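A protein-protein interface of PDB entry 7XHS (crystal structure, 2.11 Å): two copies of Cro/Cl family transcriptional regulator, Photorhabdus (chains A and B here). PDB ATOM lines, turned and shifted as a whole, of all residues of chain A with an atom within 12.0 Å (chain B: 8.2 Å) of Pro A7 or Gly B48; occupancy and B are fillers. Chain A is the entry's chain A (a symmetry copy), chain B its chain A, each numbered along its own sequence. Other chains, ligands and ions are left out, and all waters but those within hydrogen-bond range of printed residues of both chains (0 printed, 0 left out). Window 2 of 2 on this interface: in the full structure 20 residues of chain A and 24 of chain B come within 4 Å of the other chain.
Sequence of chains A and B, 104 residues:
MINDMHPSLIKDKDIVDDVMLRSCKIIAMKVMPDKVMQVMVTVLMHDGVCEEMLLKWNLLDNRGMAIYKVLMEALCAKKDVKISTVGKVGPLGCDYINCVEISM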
ATOM      1  N   ASP A   4      17.823 -24.148 -33.621  1.00  0.00           N
ATOM      2  CA  ASP A   4      16.467 -24.646 -33.427  1.00  0.00           C
ATOM      3  C   ASP A   4      16.273 -25.014 -31.962  1.00  0.00           C
ATOM      4  O   ASP A   4      16.764 -26.025 -31.483  1.00  0.00           O
ATOM      5  CB  ASP A   4      16.192 -25.846 -34.331  1.00  0.00           C
ATOM      6  CG  ASP A   4      14.715 -26.203 -34.400  1.00  0.00           C
ATOM      7  OD1 ASP A   4      14.397 -27.341 -34.824  1.00  0.00           O
ATOM      8  OD2 ASP A   4      13.880 -25.349 -34.031  1.00  0.00           O
ATOM      9  N   MET A   5      15.545 -24.174 -31.253  1.00  0.00           N
ATOM     10  CA  MET A   5      15.446 -24.275 -29.814  1.00  0.00           C
ATOM     11  C   MET A   5      14.226 -25.094 -29.431  1.00  0.00           C
ATOM     12  O   MET A   5      13.496 -25.591 -30.288  1.00  0.00           O
ATOM     13  CB  MET A   5      15.422 -22.879 -29.210  1.00  0.00           C
ATOM     14  CG  MET A   5      16.538 -22.031 -29.790  1.00  0.00           C
ATOM     15  SD  MET A   5      17.225 -21.010 -28.501  1.00  0.00           S
ATOM     16  CE  MET A   5      15.902 -19.825 -28.307  1.00  0.00           C
ATOM     17  N   HIS A   6      14.038 -25.279 -28.126  1.00  0.00           N
ATOM     18  CA  HIS A   6      12.851 -25.973 -27.663  1.00  0.00           C
ATOM     19  C   HIS A   6      11.619 -25.268 -28.211  1.00  0.00           C
ATOM     20  O   HIS A   6      11.563 -24.030 -28.206  1.00  0.00           O
ATOM     21  CB  HIS A   6      12.787 -26.011 -26.134  1.00  0.00           C
ATOM     22  CG  HIS A   6      11.823 -27.023 -25.603  1.00  0.00           C
ATOM     23  ND1 HIS A   6      10.486 -26.745 -25.402  1.00  0.00           N
ATOM     24  CD2 HIS A   6      11.995 -28.317 -25.247  1.00  0.00           C
ATOM     25  CE1 HIS A   6       9.880 -27.822 -24.936  1.00  0.00           C
ATOM     26  NE2 HIS A   6      10.770 -28.793 -24.840  1.00  0.00           N
ATOM     27  N   PRO A   7      10.634 -26.017 -28.719  1.00  0.00           N
ATOM     28  CA  PRO A   7       9.371 -25.431 -29.196  1.00  0.00           C
ATOM     29  C   PRO A   7       8.771 -24.349 -28.307  1.00  0.00           C
ATOM     30  O   PRO A   7       8.141 -23.414 -28.807  1.00  0.00           O
ATOM     31  CB  PRO A   7       8.440 -26.643 -29.243  1.00  0.00           C
ATOM     32  CG  PRO A   7       9.331 -27.778 -29.531  1.00  0.00           C
ATOM     33  CD  PRO A   7      10.671 -27.477 -28.903  1.00  0.00           C
ATOM     34  N   SER A   8       8.935 -24.472 -26.993  1.00  0.00           N
ATOM     35  CA  SER A   8       8.309 -23.553 -26.055  1.00  0.00           C
ATOM     36  C   SER A   8       9.220 -22.392 -25.646  1.00  0.00           C
ATOM     37  O   SER A   8       8.827 -21.588 -24.795  1.00  0.00           O
ATOM     38  CB  SER A   8       7.845 -24.313 -24.814  1.00  0.00           C
ATOM     39  OG  SER A   8       8.937 -24.683 -23.987  1.00  0.00           O
ATOM     40  N   LEU A   9      10.406 -22.276 -26.233  1.00  0.00           N
ATOM     41  CA  LEU A   9      11.392 -21.279 -25.831  1.00  0.00           C
ATOM     42  C   LEU A   9      11.489 -20.200 -26.901  1.00  0.00           C
ATOM     43  O   LEU A   9      11.839 -20.485 -28.052  1.00  0.00           O
ATOM     44  CB  LEU A   9      12.750 -21.936 -25.581  1.00  0.00           C
ATOM     45  CG  LEU A   9      13.930 -21.049 -25.172  1.00  0.00           C
ATOM     46  CD1 LEU A   9      13.507 -20.042 -24.144  1.00  0.00           C
ATOM     47  CD2 LEU A   9      15.065 -21.898 -24.640  1.00  0.00           C
ATOM     48  N   ILE A  10      11.192 -18.965 -26.510  1.00  0.00           N
ATOM     49  CA  ILE A  10      11.211 -17.835 -27.433  1.00  0.00           C
ATOM     50  C   ILE A  10      12.631 -17.567 -27.932  1.00  0.00           C
ATOM     51  O   ILE A  10      13.622 -17.859 -27.247  1.00  0.00           O
ATOM     52  CB  ILE A  10      10.636 -16.590 -26.730  1.00  0.00           C
ATOM     53  CG1 ILE A  10      10.346 -15.478 -27.731  1.00  0.00           C
ATOM     54  CG2 ILE A  10      11.614 -16.079 -25.655  1.00  0.00           C
ATOM     55  CD1 ILE A  10       9.513 -14.366 -27.144  1.00  0.00           C
ATOM     56  N   LYS A  11      12.715 -16.976 -29.127  1.00  0.00           N
ATOM     57  CA  LYS A  11      13.941 -16.541 -29.816  1.00  0.00           C
ATOM     58  C   LYS A  11      14.543 -17.695 -30.607  1.00  0.00           C
ATOM     59  O   LYS A  11      15.644 -17.584 -31.147  1.00  0.00           O
ATOM     60  CB  LYS A  11      14.992 -15.959 -28.852  1.00  0.00           C
ATOM     61  CG  LYS A  11      14.542 -14.718 -28.107  1.00  0.00           C
ATOM     62  CD  LYS A  11      15.515 -14.386 -26.984  1.00  0.00           C
ATOM     63  CE  LYS A  11      16.485 -13.291 -27.394  1.00  0.00           C
ATOM     64  NZ  LYS A  11      17.660 -13.247 -26.486  1.00  0.00           N
ATOM     65  N   SER A 103       5.821 -11.905 -23.836  1.00  0.00           N
ATOM     66  CA  SER A 103       5.797 -13.359 -23.947  1.00  0.00           C
ATOM     67  C   SER A 103       5.192 -14.008 -22.705  1.00  0.00           C
ATOM     68  O   SER A 103       5.258 -13.466 -21.596  1.00  0.00           O
ATOM     69  CB  SER A 103       7.200 -13.914 -24.231  1.00  0.00           C
ATOM     70  OG  SER A 103       8.024 -13.783 -23.115  1.00  0.00           O
ATOM     71  N   MET A 104       4.587 -15.177 -22.911  1.00  0.00           N
ATOM     72  CA  MET A 104       3.929 -15.912 -21.829  1.00  0.00           C
ATOM     73  C   MET A 104       4.885 -16.287 -20.712  1.00  0.00           C
ATOM     74  O   MET A 104       6.013 -16.721 -20.954  1.00  0.00           O
ATOM     75  CB  MET A 104       3.284 -17.193 -22.340  1.00  0.00           C
ATOM     76  CG  MET A 104       2.337 -17.812 -21.326  1.00  0.00           C
ATOM     77  SD  MET A 104       1.552 -19.305 -21.958  1.00  0.00           S
ATOM     78  CE  MET A 104      -0.040 -18.635 -22.353  1.00  0.00           C
ATOM     79  OXT MET A 104       4.530 -16.172 -19.542  1.00  0.00           O
ATOM     80  N   SER B  23      -6.177 -26.766 -30.639  1.00  0.00           N
ATOM     81  CA  SER B  23      -5.799 -26.297 -29.313  1.00  0.00           C
ATOM     82  C   SER B  23      -4.328 -25.893 -29.262  1.00  0.00           C
ATOM     83  O   SER B  23      -3.462 -26.578 -29.816  1.00  0.00           O
ATOM     84  CB  SER B  23      -6.068 -27.394 -28.291  1.00  0.00           C
ATOM     85  OG  SER B  23      -5.311 -27.165 -27.121  1.00  0.00           O
ATOM     86  N   ILE B  27       2.315 -18.042 -26.923  1.00  0.00           N
ATOM     87  CA  ILE B  27       3.483 -17.900 -26.065  1.00  0.00           C
ATOM     88  C   ILE B  27       4.272 -16.614 -26.300  1.00  0.00           C
ATOM     89  O   ILE B  27       5.138 -16.287 -25.472  1.00  0.00           O
ATOM     90  CB  ILE B  27       4.403 -19.139 -26.167  1.00  0.00           C
ATOM     91  CG1 ILE B  27       4.964 -19.329 -27.577  1.00  0.00           C
ATOM     92  CG2 ILE B  27       3.637 -20.391 -25.691  1.00  0.00           C
ATOM     93  CD1 ILE B  27       6.081 -20.390 -27.650  1.00  0.00           C
ATOM     94  N   THR B  42       3.402 -15.922 -31.875  1.00  0.00           N
ATOM     95  CA  THR B  42       4.055 -17.226 -31.757  1.00  0.00           C
ATOM     96  C   THR B  42       3.149 -18.197 -31.005  1.00  0.00           C
ATOM     97  O   THR B  42       2.750 -17.929 -29.859  1.00  0.00           O
ATOM     98  CB  THR B  42       5.416 -17.094 -31.070  1.00  0.00           C
ATOM     99  OG1 THR B  42       6.198 -16.110 -31.767  1.00  0.00           O
ATOM    100  CG2 THR B  42       6.174 -18.447 -31.062  1.00  0.00           C
ATOM    101  N   VAL B  43       2.825 -19.331 -31.643  1.00  0.00           N
ATOM    102  CA  VAL B  43       1.837 -20.268 -31.105  1.00  0.00           C
ATOM    103  C   VAL B  43       2.471 -21.646 -30.916  1.00  0.00           C
ATOM    104  O   VAL B  43       3.212 -22.135 -31.777  1.00  0.00           O
ATOM    105  CB  VAL B  43       0.568 -20.356 -31.988  1.00  0.00           C
ATOM    106  CG1 VAL B  43      -0.030 -18.946 -32.245  1.00  0.00           C
ATOM    107  CG2 VAL B  43       0.844 -21.052 -33.300  1.00  0.00           C
ATOM    108  N   LEU B  44       2.178 -22.261 -29.769  1.00  0.00           N
ATOM    109  CA  LEU B  44       2.639 -23.599 -29.435  1.00  0.00           C
ATOM    110  C   LEU B  44       1.431 -24.536 -29.423  1.00  0.00           C
ATOM    111  O   LEU B  44       0.559 -24.417 -28.558  1.00  0.00           O
ATOM    112  CB  LEU B  44       3.373 -23.570 -28.097  1.00  0.00           C
ATOM    113  CG  LEU B  44       3.830 -24.885 -27.479  1.00  0.00           C
ATOM    114  CD1 LEU B  44       4.973 -25.464 -28.276  1.00  0.00           C
ATOM    115  CD2 LEU B  44       4.278 -24.611 -26.041  1.00  0.00           C
ATOM    116  N   MET B  45       1.368 -25.443 -30.408  1.00  0.00           N
ATOM    117  CA  MET B  45       0.302 -26.432 -30.505  1.00  0.00           C
ATOM    118  C   MET B  45       0.509 -27.539 -29.478  1.00  0.00           C
ATOM    119  O   MET B  45       1.614 -27.756 -28.975  1.00  0.00           O
ATOM    120  CB  MET B  45       0.238 -27.067 -31.901  1.00  0.00           C
ATOM    121  CG  MET B  45       0.299 -26.109 -33.089  1.00  0.00           C
ATOM    122  SD  MET B  45      -1.101 -24.974 -33.185  1.00  0.00           S
ATOM    123  CE  MET B  45      -0.765 -24.238 -34.776  1.00  0.00           C
ATOM    124  N   HIS B  46      -0.576 -28.255 -29.183  1.00  0.00           N
ATOM    125  CA  HIS B  46      -0.532 -29.307 -28.170  1.00  0.00           C
ATOM    126  C   HIS B  46       0.376 -30.480 -28.551  1.00  0.00           C
ATOM    127  O   HIS B  46       0.805 -31.230 -27.667  1.00  0.00           O
ATOM    128  CB  HIS B  46      -1.946 -29.815 -27.891  1.00  0.00           C
ATOM    129  CG  HIS B  46      -2.135 -30.336 -26.500  1.00  0.00           C
ATOM    130  ND1 HIS B  46      -2.022 -29.533 -25.384  1.00  0.00           N
ATOM    131  CD2 HIS B  46      -2.437 -31.577 -26.044  1.00  0.00           C
ATOM    132  CE1 HIS B  46      -2.239 -30.259 -24.300  1.00  0.00           C
ATOM    133  NE2 HIS B  46      -2.496 -31.501 -24.673  1.00  0.00           N
ATOM    134  N   ASP B  47       0.685 -30.665 -29.831  1.00  0.00           N
ATOM    135  CA  ASP B  47       1.557 -31.756 -30.246  1.00  0.00           C
ATOM    136  C   ASP B  47       3.021 -31.339 -30.351  1.00  0.00           C
ATOM    137  O   ASP B  47       3.821 -32.057 -30.961  1.00  0.00           O
ATOM    138  CB  ASP B  47       1.074 -32.334 -31.577  1.00  0.00           C
ATOM    139  CG  ASP B  47       1.247 -31.369 -32.742  1.00  0.00           C
ATOM    140  OD1 ASP B  47       0.936 -31.773 -33.884  1.00  0.00           O
ATOM    141  OD2 ASP B  47       1.686 -30.212 -32.535  1.00  0.00           O
ATOM    142  N   GLY B  48       3.388 -30.190 -29.800  1.00  0.00           N
ATOM    143  CA  GLY B  48       4.779 -29.822 -29.699  1.00  0.00           C
ATOM    144  C   GLY B  48       5.327 -28.955 -30.813  1.00  0.00           C
ATOM    145  O   GLY B  48       6.446 -28.456 -30.680  1.00  0.00           O
ATOM    146  N   VAL B  49       4.596 -28.752 -31.902  1.00  0.00           N
ATOM    147  CA  VAL B  49       5.104 -27.895 -32.968  1.00  0.00           C
ATOM    148  C   VAL B  49       4.811 -26.432 -32.637  1.00  0.00           C
ATOM    149  O   VAL B  49       3.769 -26.093 -32.060  1.00  0.00           O
ATOM    150  CB  VAL B  49       4.517 -28.312 -34.326  1.00  0.00           C
ATOM    151  CG1 VAL B  49       4.799 -29.790 -34.580  1.00  0.00           C
ATOM    152  CG2 VAL B  49       3.036 -28.044 -34.383  1.00  0.00           C
ATOM    153  N   CYS B  50       5.751 -25.558 -32.976  1.00  0.00           N
ATOM    154  CA  CYS B  50       5.645 -24.131 -32.721  1.00  0.00           C
ATOM    155  C   CYS B  50       5.615 -23.398 -34.056  1.00  0.00           C
ATOM    156  O   CYS B  50       6.385 -23.727 -34.962  1.00  0.00           O
ATOM    157  CB  CYS B  50       6.819 -23.670 -31.861  1.00  0.00           C
ATOM    158  SG  CYS B  50       6.848 -21.913 -31.496  1.00  0.00           S
ATOM    159  N   GLU B  51       4.718 -22.417 -34.189  1.00  0.00           N
ATOM    160  CA  GLU B  51       4.457 -21.761 -35.469  1.00  0.00           C
ATOM    161  C   GLU B  51       4.306 -20.257 -35.291  1.00  0.00           C
ATOM    162  O   GLU B  51       3.703 -19.811 -34.314  1.00  0.00           O
ATOM    163  CB  GLU B  51       3.174 -22.297 -36.115  1.00  0.00           C
ATOM    164  CG  GLU B  51       3.115 -22.097 -37.607  1.00  0.00           C
ATOM    165  CD  GLU B  51       2.066 -22.975 -38.270  1.00  0.00           C
ATOM    166  OE1 GLU B  51       1.435 -22.507 -39.242  1.00  0.00           O
ATOM    167  OE2 GLU B  51       1.856 -24.121 -37.805  1.00  0.00           O
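No position is printed for both chains.
Among the printed residues, pairs that only touch across the chains: Pro A7 with Gly B48, Ser A103 with Ile B27, Ser A8 with Leu B44, Pro A7 with Leu B44 and Pro A7 with Ile B27.
N of Ile B27 lies within hydrogen-bond range of O of Thr B42 (3.0 Å). The side-chain sulfur (SG) of Cys B50 sits close to the backbone carbonyl oxygen (O) of Val B43, at 3.7 Å. A ring nitrogen (ND1) of His A6 is in hydrogen-bond range of the side-chain hydroxyl (OG) of Ser A8, at 2.9 Å.
Of chain A, only Pro A7 (3.1 Å) comes within 4 Å of Gly B48. No residue of chain A comes within 4 Å of Asp B47. No residue of chain A comes within 4 Å of Val B49. Printed residues of chain B within 4 Å of Ser A8: Leu B44 (3.8 Å). Of the printed residues of chain B, Met A104 touches Ile B27 (2.8 Å). Ser B23 touches none of the printed residues of chain A. The nearest residue of chain A that does not touch Gly B48 is Ser A8 (6.0 Å). The nearest printed residue of chain B that does not touch Ser A8 is Ile B27 (4.1 Å).
Of the 12 printed residues of chain B, 4 touch a printed residue of chain A. Hydrophobic or aromatic side chains of chain B within 4 Å of the printed part of chain A: Ile B27 and Leu B44. Of the 10 printed residues of chain A, 4 touch a printed residue of chain B. Among the printed residues, 7 pairs touch across the chains.
The backbone carbonyl oxygen (O) of Ile B27 sits at hydrogen-bond distance from the backbone NH (N) of Met A104 (2.8 Å). The side-chain sulfur of Cys B50 lies close to the backbone carbonyl oxygen of Pro A7.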
